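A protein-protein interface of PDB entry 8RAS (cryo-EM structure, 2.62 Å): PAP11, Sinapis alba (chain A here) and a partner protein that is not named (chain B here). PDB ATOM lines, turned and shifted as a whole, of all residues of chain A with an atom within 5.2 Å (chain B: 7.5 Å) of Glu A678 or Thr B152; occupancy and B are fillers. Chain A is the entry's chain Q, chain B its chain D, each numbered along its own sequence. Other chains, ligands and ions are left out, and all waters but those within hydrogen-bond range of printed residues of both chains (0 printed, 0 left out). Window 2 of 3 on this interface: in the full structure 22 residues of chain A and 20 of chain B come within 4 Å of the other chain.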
ATOM      1  N   LEU A 674       1.816  -4.702  10.256  1.00  0.00           N
ATOM      2  CA  LEU A 674       0.914  -4.435   9.144  1.00  0.00           C
ATOM      3  C   LEU A 674       0.377  -3.014   9.194  1.00  0.00           C
ATOM      4  O   LEU A 674       0.134  -2.408   8.145  1.00  0.00           O
ATOM      5  CB  LEU A 674      -0.230  -5.446   9.149  1.00  0.00           C
ATOM      6  CG  LEU A 674       0.122  -6.795   8.523  1.00  0.00           C
ATOM      7  CD1 LEU A 674      -0.789  -7.897   9.041  1.00  0.00           C
ATOM      8  CD2 LEU A 674       0.057  -6.707   7.014  1.00  0.00           C
ATOM      9  N   LYS A 675       0.181  -2.468  10.397  1.00  0.00           N
ATOM     10  CA  LYS A 675      -0.169  -1.057  10.507  1.00  0.00           C
ATOM     11  C   LYS A 675       0.967  -0.187   9.981  1.00  0.00           C
ATOM     12  O   LYS A 675       0.728   0.850   9.351  1.00  0.00           O
ATOM     13  CB  LYS A 675      -0.501  -0.714  11.964  1.00  0.00           C
ATOM     14  CG  LYS A 675      -0.663   0.778  12.355  1.00  0.00           C
ATOM     15  CD  LYS A 675      -1.379   1.741  11.371  1.00  0.00           C
ATOM     16  CE  LYS A 675      -2.575   1.146  10.620  1.00  0.00           C
ATOM     17  NZ  LYS A 675      -3.568   0.530  11.543  1.00  0.00           N
ATOM     18  N   HIS A 676       2.214  -0.602  10.223  1.00  0.00           N
ATOM     19  CA  HIS A 676       3.347   0.075   9.603  1.00  0.00           C
ATOM     20  C   HIS A 676       3.274  -0.021   8.083  1.00  0.00           C
ATOM     21  O   HIS A 676       3.543   0.959   7.378  1.00  0.00           O
ATOM     22  CB  HIS A 676       4.661  -0.521  10.110  1.00  0.00           C
ATOM     23  CG  HIS A 676       4.959  -0.203  11.543  1.00  0.00           C
ATOM     24  ND1 HIS A 676       4.766   1.051  12.083  1.00  0.00           N
ATOM     25  CD2 HIS A 676       5.442  -0.974  12.545  1.00  0.00           C
ATOM     26  CE1 HIS A 676       5.114   1.037  13.357  1.00  0.00           C
ATOM     27  NE2 HIS A 676       5.527  -0.179  13.662  1.00  0.00           N
ATOM     28  N   GLY A 677       2.909  -1.195   7.562  1.00  0.00           N
ATOM     29  CA  GLY A 677       2.814  -1.360   6.120  1.00  0.00           C
ATOM     30  C   GLY A 677       1.730  -0.502   5.496  1.00  0.00           C
ATOM     31  O   GLY A 677       1.903   0.028   4.395  1.00  0.00           O
ATOM     32  N   GLU A 678       0.594  -0.360   6.184  1.00  0.00           N
ATOM     33  CA  GLU A 678      -0.487   0.468   5.662  1.00  0.00           C
ATOM     34  C   GLU A 678      -0.047   1.920   5.512  1.00  0.00           C
ATOM     35  O   GLU A 678      -0.360   2.572   4.510  1.00  0.00           O
ATOM     36  CB  GLU A 678      -1.710   0.371   6.571  1.00  0.00           C
ATOM     37  CG  GLU A 678      -2.785   1.400   6.273  1.00  0.00           C
ATOM     38  CD  GLU A 678      -4.162   0.783   6.169  1.00  0.00           C
ATOM     39  OE1 GLU A 678      -4.398  -0.255   6.822  1.00  0.00           O
ATOM     40  OE2 GLU A 678      -5.009   1.332   5.435  1.00  0.00           O
ATOM     41  N   HIS A 679       0.682   2.439   6.496  1.00  0.00           N
ATOM     42  CA  HIS A 679       1.212   3.795   6.435  1.00  0.00           C
ATOM     43  C   HIS A 679       2.466   3.901   5.575  1.00  0.00           C
ATOM     44  O   HIS A 679       3.124   4.946   5.606  1.00  0.00           O
ATOM     45  CB  HIS A 679       1.507   4.308   7.846  1.00  0.00           C
ATOM     46  CG  HIS A 679       0.345   4.994   8.493  1.00  0.00           C
ATOM     47  ND1 HIS A 679      -0.532   5.792   7.791  1.00  0.00           N
ATOM     48  CD2 HIS A 679      -0.082   5.004   9.778  1.00  0.00           C
ATOM     49  CE1 HIS A 679      -1.451   6.263   8.615  1.00  0.00           C
ATOM     50  NE2 HIS A 679      -1.201   5.800   9.827  1.00  0.00           N
ATOM     51  N   ASP A 680       2.798   2.843   4.827  1.00  0.00           N
ATOM     52  CA  ASP A 680       3.948   2.766   3.926  1.00  0.00           C
ATOM     53  C   ASP A 680       5.210   3.380   4.525  1.00  0.00           C
ATOM     54  O   ASP A 680       5.994   4.018   3.816  1.00  0.00           O
ATOM     55  CB  ASP A 680       3.626   3.411   2.570  1.00  0.00           C
ATOM     56  CG  ASP A 680       3.174   4.856   2.687  1.00  0.00           C
ATOM     57  OD1 ASP A 680       3.999   5.721   3.049  1.00  0.00           O
ATOM     58  OD2 ASP A 680       1.986   5.129   2.414  1.00  0.00           O
ATOM     59  N   ARG B 149      -3.738  -2.022  -3.682  1.00  0.00           N
ATOM     60  CA  ARG B 149      -3.850  -2.383  -2.272  1.00  0.00           C
ATOM     61  C   ARG B 149      -5.294  -2.713  -1.911  1.00  0.00           C
ATOM     62  O   ARG B 149      -5.949  -1.940  -1.202  1.00  0.00           O
ATOM     63  CB  ARG B 149      -3.320  -1.260  -1.378  1.00  0.00           C
ATOM     64  CG  ARG B 149      -2.955  -1.709   0.028  1.00  0.00           C
ATOM     65  CD  ARG B 149      -2.355  -0.568   0.830  1.00  0.00           C
ATOM     66  NE  ARG B 149      -1.517   0.294   0.006  1.00  0.00           N
ATOM     67  CZ  ARG B 149      -0.216   0.470   0.190  1.00  0.00           C
ATOM     68  NH1 ARG B 149       0.434  -0.147   1.164  1.00  0.00           N
ATOM     69  NH2 ARG B 149       0.450   1.285  -0.623  1.00  0.00           N
ATOM     70  N   PRO B 150      -5.829  -3.843  -2.387  1.00  0.00           N
ATOM     71  CA  PRO B 150      -7.213  -4.194  -2.043  1.00  0.00           C
ATOM     72  C   PRO B 150      -7.364  -4.819  -0.669  1.00  0.00           C
ATOM     73  O   PRO B 150      -8.456  -4.736  -0.090  1.00  0.00           O
ATOM     74  CB  PRO B 150      -7.596  -5.188  -3.143  1.00  0.00           C
ATOM     75  CG  PRO B 150      -6.307  -5.888  -3.445  1.00  0.00           C
ATOM     76  CD  PRO B 150      -5.186  -4.892  -3.198  1.00  0.00           C
ATOM     77  N   ILE B 151      -6.316  -5.440  -0.126  1.00  0.00           N
ATOM     78  CA  ILE B 151      -6.393  -6.135   1.150  1.00  0.00           C
ATOM     79  C   ILE B 151      -5.297  -5.618   2.069  1.00  0.00           C
ATOM     80  O   ILE B 151      -4.295  -5.050   1.627  1.00  0.00           O
ATOM     81  CB  ILE B 151      -6.292  -7.668   0.985  1.00  0.00           C
ATOM     82  CG1 ILE B 151      -4.833  -8.114   0.943  1.00  0.00           C
ATOM     83  CG2 ILE B 151      -7.028  -8.133  -0.263  1.00  0.00           C
ATOM     84  CD1 ILE B 151      -4.654  -9.574   1.239  1.00  0.00           C
ATOM     85  N   THR B 152      -5.504  -5.813   3.365  1.00  0.00           N
ATOM     86  CA  THR B 152      -4.621  -5.266   4.390  1.00  0.00           C
ATOM     87  C   THR B 152      -4.099  -6.318   5.359  1.00  0.00           C
ATOM     88  O   THR B 152      -2.946  -6.229   5.789  1.00  0.00           O
ATOM     89  CB  THR B 152      -5.357  -4.154   5.163  1.00  0.00           C
ATOM     90  OG1 THR B 152      -5.714  -3.101   4.260  1.00  0.00           O
ATOM     91  CG2 THR B 152      -4.479  -3.585   6.266  1.00  0.00           C
ATOM     92  N   LYS B 153      -4.902  -7.329   5.691  1.00  0.00           N
ATOM     93  CA  LYS B 153      -4.503  -8.326   6.680  1.00  0.00           C
ATOM     94  C   LYS B 153      -3.368  -9.227   6.208  1.00  0.00           C
ATOM     95  O   LYS B 153      -3.014 -10.166   6.929  1.00  0.00           O
ATOM     96  CB  LYS B 153      -5.708  -9.179   7.080  1.00  0.00           C
ATOM     97  CG  LYS B 153      -6.763  -8.422   7.871  1.00  0.00           C
ATOM     98  CD  LYS B 153      -7.935  -9.316   8.226  1.00  0.00           C
ATOM     99  CE  LYS B 153      -9.074  -8.510   8.826  1.00  0.00           C
ATOM    100  NZ  LYS B 153      -8.590  -7.545   9.851  1.00  0.00           N
ATOM    101  N   LYS B 154      -2.799  -8.980   5.029  1.00  0.00           N
ATOM    102  CA  LYS B 154      -1.621  -9.690   4.562  1.00  0.00           C
ATOM    103  C   LYS B 154      -0.571  -8.679   4.120  1.00  0.00           C
ATOM    104  O   LYS B 154      -0.914  -7.628   3.565  1.00  0.00           O
ATOM    105  CB  LYS B 154      -1.964 -10.636   3.401  1.00  0.00           C
ATOM    106  CG  LYS B 154      -3.116 -11.586   3.694  1.00  0.00           C
ATOM    107  CD  LYS B 154      -2.720 -12.658   4.694  1.00  0.00           C
ATOM    108  CE  LYS B 154      -2.366 -13.957   3.992  1.00  0.00           C
ATOM    109  NZ  LYS B 154      -3.580 -14.734   3.616  1.00  0.00           N
ATOM    110  N   PRO B 155       0.708  -8.961   4.359  1.00  0.00           N
ATOM    111  CA  PRO B 155       1.749  -7.971   4.062  1.00  0.00           C
ATOM    112  C   PRO B 155       1.917  -7.725   2.571  1.00  0.00           C
ATOM    113  O   PRO B 155       1.707  -8.611   1.738  1.00  0.00           O
ATOM    114  CB  PRO B 155       3.013  -8.596   4.664  1.00  0.00           C
ATOM    115  CG  PRO B 155       2.726 -10.055   4.724  1.00  0.00           C
ATOM    116  CD  PRO B 155       1.256 -10.179   4.979  1.00  0.00           C
ATOM    117  N   THR B 156       2.306  -6.494   2.244  1.00  0.00           N
ATOM    118  CA  THR B 156       2.614  -6.071   0.883  1.00  0.00           C
ATOM    119  C   THR B 156       3.982  -5.398   0.874  1.00  0.00           C
ATOM    120  O   THR B 156       4.605  -5.195   1.921  1.00  0.00           O
ATOM    121  CB  THR B 156       1.543  -5.119   0.331  1.00  0.00           C
ATOM    122  OG1 THR B 156       1.626  -3.859   1.008  1.00  0.00           O
ATOM    123  CG2 THR B 156       0.151  -5.703   0.519  1.00  0.00           C
ATOM    124  N   ARG B 161      -1.234   2.938  -4.345  1.00  0.00           N
ATOM    125  CA  ARG B 161      -2.425   3.342  -3.613  1.00  0.00           C
ATOM    126  C   ARG B 161      -3.397   4.011  -4.572  1.00  0.00           C
ATOM    127  O   ARG B 161      -3.018   4.487  -5.644  1.00  0.00           O
ATOM    128  CB  ARG B 161      -2.085   4.278  -2.444  1.00  0.00           C
ATOM    129  CG  ARG B 161      -2.093   5.755  -2.797  1.00  0.00           C
ATOM    130  CD  ARG B 161      -1.783   6.608  -1.578  1.00  0.00           C
ATOM    131  NE  ARG B 161      -0.443   6.357  -1.061  1.00  0.00           N
ATOM    132  CZ  ARG B 161       0.603   7.144  -1.275  1.00  0.00           C
ATOM    133  NH1 ARG B 161       0.502   8.248  -1.997  1.00  0.00           N
ATOM    134  NH2 ARG B 161       1.780   6.814  -0.750  1.00  0.00           N
ATOM    135  N   ARG B 190      -3.001  -9.635  -4.028  1.00  0.00           N
ATOM    136  CA  ARG B 190      -2.787  -9.019  -2.726  1.00  0.00           C
ATOM    137  C   ARG B 190      -2.342  -7.566  -2.795  1.00  0.00           C
ATOM    138  O   ARG B 190      -2.362  -6.894  -1.760  1.00  0.00           O
ATOM    139  CB  ARG B 190      -1.756  -9.820  -1.919  1.00  0.00           C
ATOM    140  CG  ARG B 190      -2.327 -11.067  -1.262  1.00  0.00           C
ATOM    141  CD  ARG B 190      -1.229 -12.020  -0.830  1.00  0.00           C
ATOM    142  NE  ARG B 190      -0.389 -11.445   0.212  1.00  0.00           N
ATOM    143  CZ  ARG B 190       0.391 -12.150   1.021  1.00  0.00           C
ATOM    144  NH1 ARG B 190       0.462 -13.468   0.935  1.00  0.00           N
ATOM    145  NH2 ARG B 190       1.115 -11.517   1.937  1.00  0.00           N
ATOM    146  N   GLU B 201     -12.863  -8.750  -1.720  1.00  0.00           N
ATOM    147  CA  GLU B 201     -11.693  -8.793  -0.849  1.00  0.00           C
ATOM    148  C   GLU B 201     -11.676  -7.611   0.114  1.00  0.00           C
ATOM    149  O   GLU B 201     -11.326  -7.766   1.290  1.00  0.00           O
ATOM    150  CB  GLU B 201     -10.416  -8.822  -1.686  1.00  0.00           C
ATOM    151  CG  GLU B 201     -10.204 -10.120  -2.448  1.00  0.00           C
ATOM    152  CD  GLU B 201     -10.303 -11.341  -1.559  1.00  0.00           C
ATOM    153  OE1 GLU B 201      -9.560 -11.414  -0.558  1.00  0.00           O
ATOM    154  OE2 GLU B 201     -11.127 -12.232  -1.863  1.00  0.00           O
ATOM    155  N   GLN B 202     -12.042  -6.421  -0.368  1.00  0.00           N
ATOM    156  CA  GLN B 202     -12.097  -5.255   0.507  1.00  0.00           C
ATOM    157  C   GLN B 202     -13.168  -5.415   1.579  1.00  0.00           C
ATOM    158  O   GLN B 202     -12.975  -5.002   2.728  1.00  0.00           O
ATOM    159  CB  GLN B 202     -12.353  -3.990  -0.312  1.00  0.00           C
ATOM    160  CG  GLN B 202     -11.212  -3.596  -1.229  1.00  0.00           C
ATOM    161  CD  GLN B 202     -11.591  -2.485  -2.185  1.00  0.00           C
ATOM    162  OE1 GLN B 202     -11.904  -1.370  -1.766  1.00  0.00           O
ATOM    163  NE2 GLN B 202     -11.568  -2.782  -3.478  1.00  0.00           N
ATOM    164  N   ASP B 205     -12.162  -8.264   4.563  1.00  0.00           N
ATOM    165  CA  ASP B 205     -11.174  -7.925   5.578  1.00  0.00           C
ATOM    166  C   ASP B 205     -11.485  -6.621   6.303  1.00  0.00           C
ATOM    167  O   ASP B 205     -10.648  -6.143   7.076  1.00  0.00           O
ATOM    168  CB  ASP B 205      -9.776  -7.855   4.958  1.00  0.00           C
ATOM    169  CG  ASP B 205      -9.652  -6.772   3.905  1.00  0.00           C
ATOM    170  OD1 ASP B 205     -10.670  -6.137   3.567  1.00  0.00           O
ATOM    171  OD2 ASP B 205      -8.527  -6.548   3.420  1.00  0.00           O
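NH2 of Arg B161 is in salt-bridge range of OD2 of Asp A680 (3.6 Å).
The backbone NH of Thr B152 lies within hydrogen-bond range of the side-chain carboxylate of Asp B205 (3.1 Å). The guanidinium group (NH2) of Arg B190 lies within hydrogen-bond range of the backbone carbonyl oxygen (O) of Pro B155, 3.0 Å away.
Leu A674 touches Thr B152. Lys B153 touches Leu A674. Leu A674 touches Lys B154. CD2 of Leu A674 touches N of Pro B155 (3.5 Å). Gly A677 touches Arg B149. Glu A678 touches Thr B152.
Thr B152 touches just these residues of chain A: Leu A674 (3.3 Å) and Glu A678 (3.4 Å). Gly A677 touches one residue of chain B. Of the printed residues of chain A, Arg B161 touches Asp A680. Printed residues of chain A within 4 Å of Lys B154: Leu A674. Of the printed residues of chain A, Pro B155 touches Leu A674 (3.5 Å). Printed residues of chain B within 4 Å of Leu A674: Thr B152 (3.3 Å), Lys B153 (3.8 Å), Lys B154 (3.6 Å) and Pro B155 (3.5 Å). Asp B205 touches none of the printed residues of chain A. Arg B190 touches none of the printed residues of chain A. The nearest residue of chain B that does not touch Glu A678 is Arg B149 (4.4 Å). The nearest printed residue of chain A that does not touch Thr B152 is Lys A675 (6.3 Å).
Printed residues of chain A that touch a printed residue of chain B: Leu A674, Gly A677, Glu A678 and Asp A680. Hydrophobic or aromatic side chains of chain A that line the printed part of chain B: Leu A674. Among the printed residues, Asp or Glu carboxylates within 4 Å of a Lys or Arg side-chain nitrogen of the other chain: Asp A680 with Arg B161 (3.6 Å).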
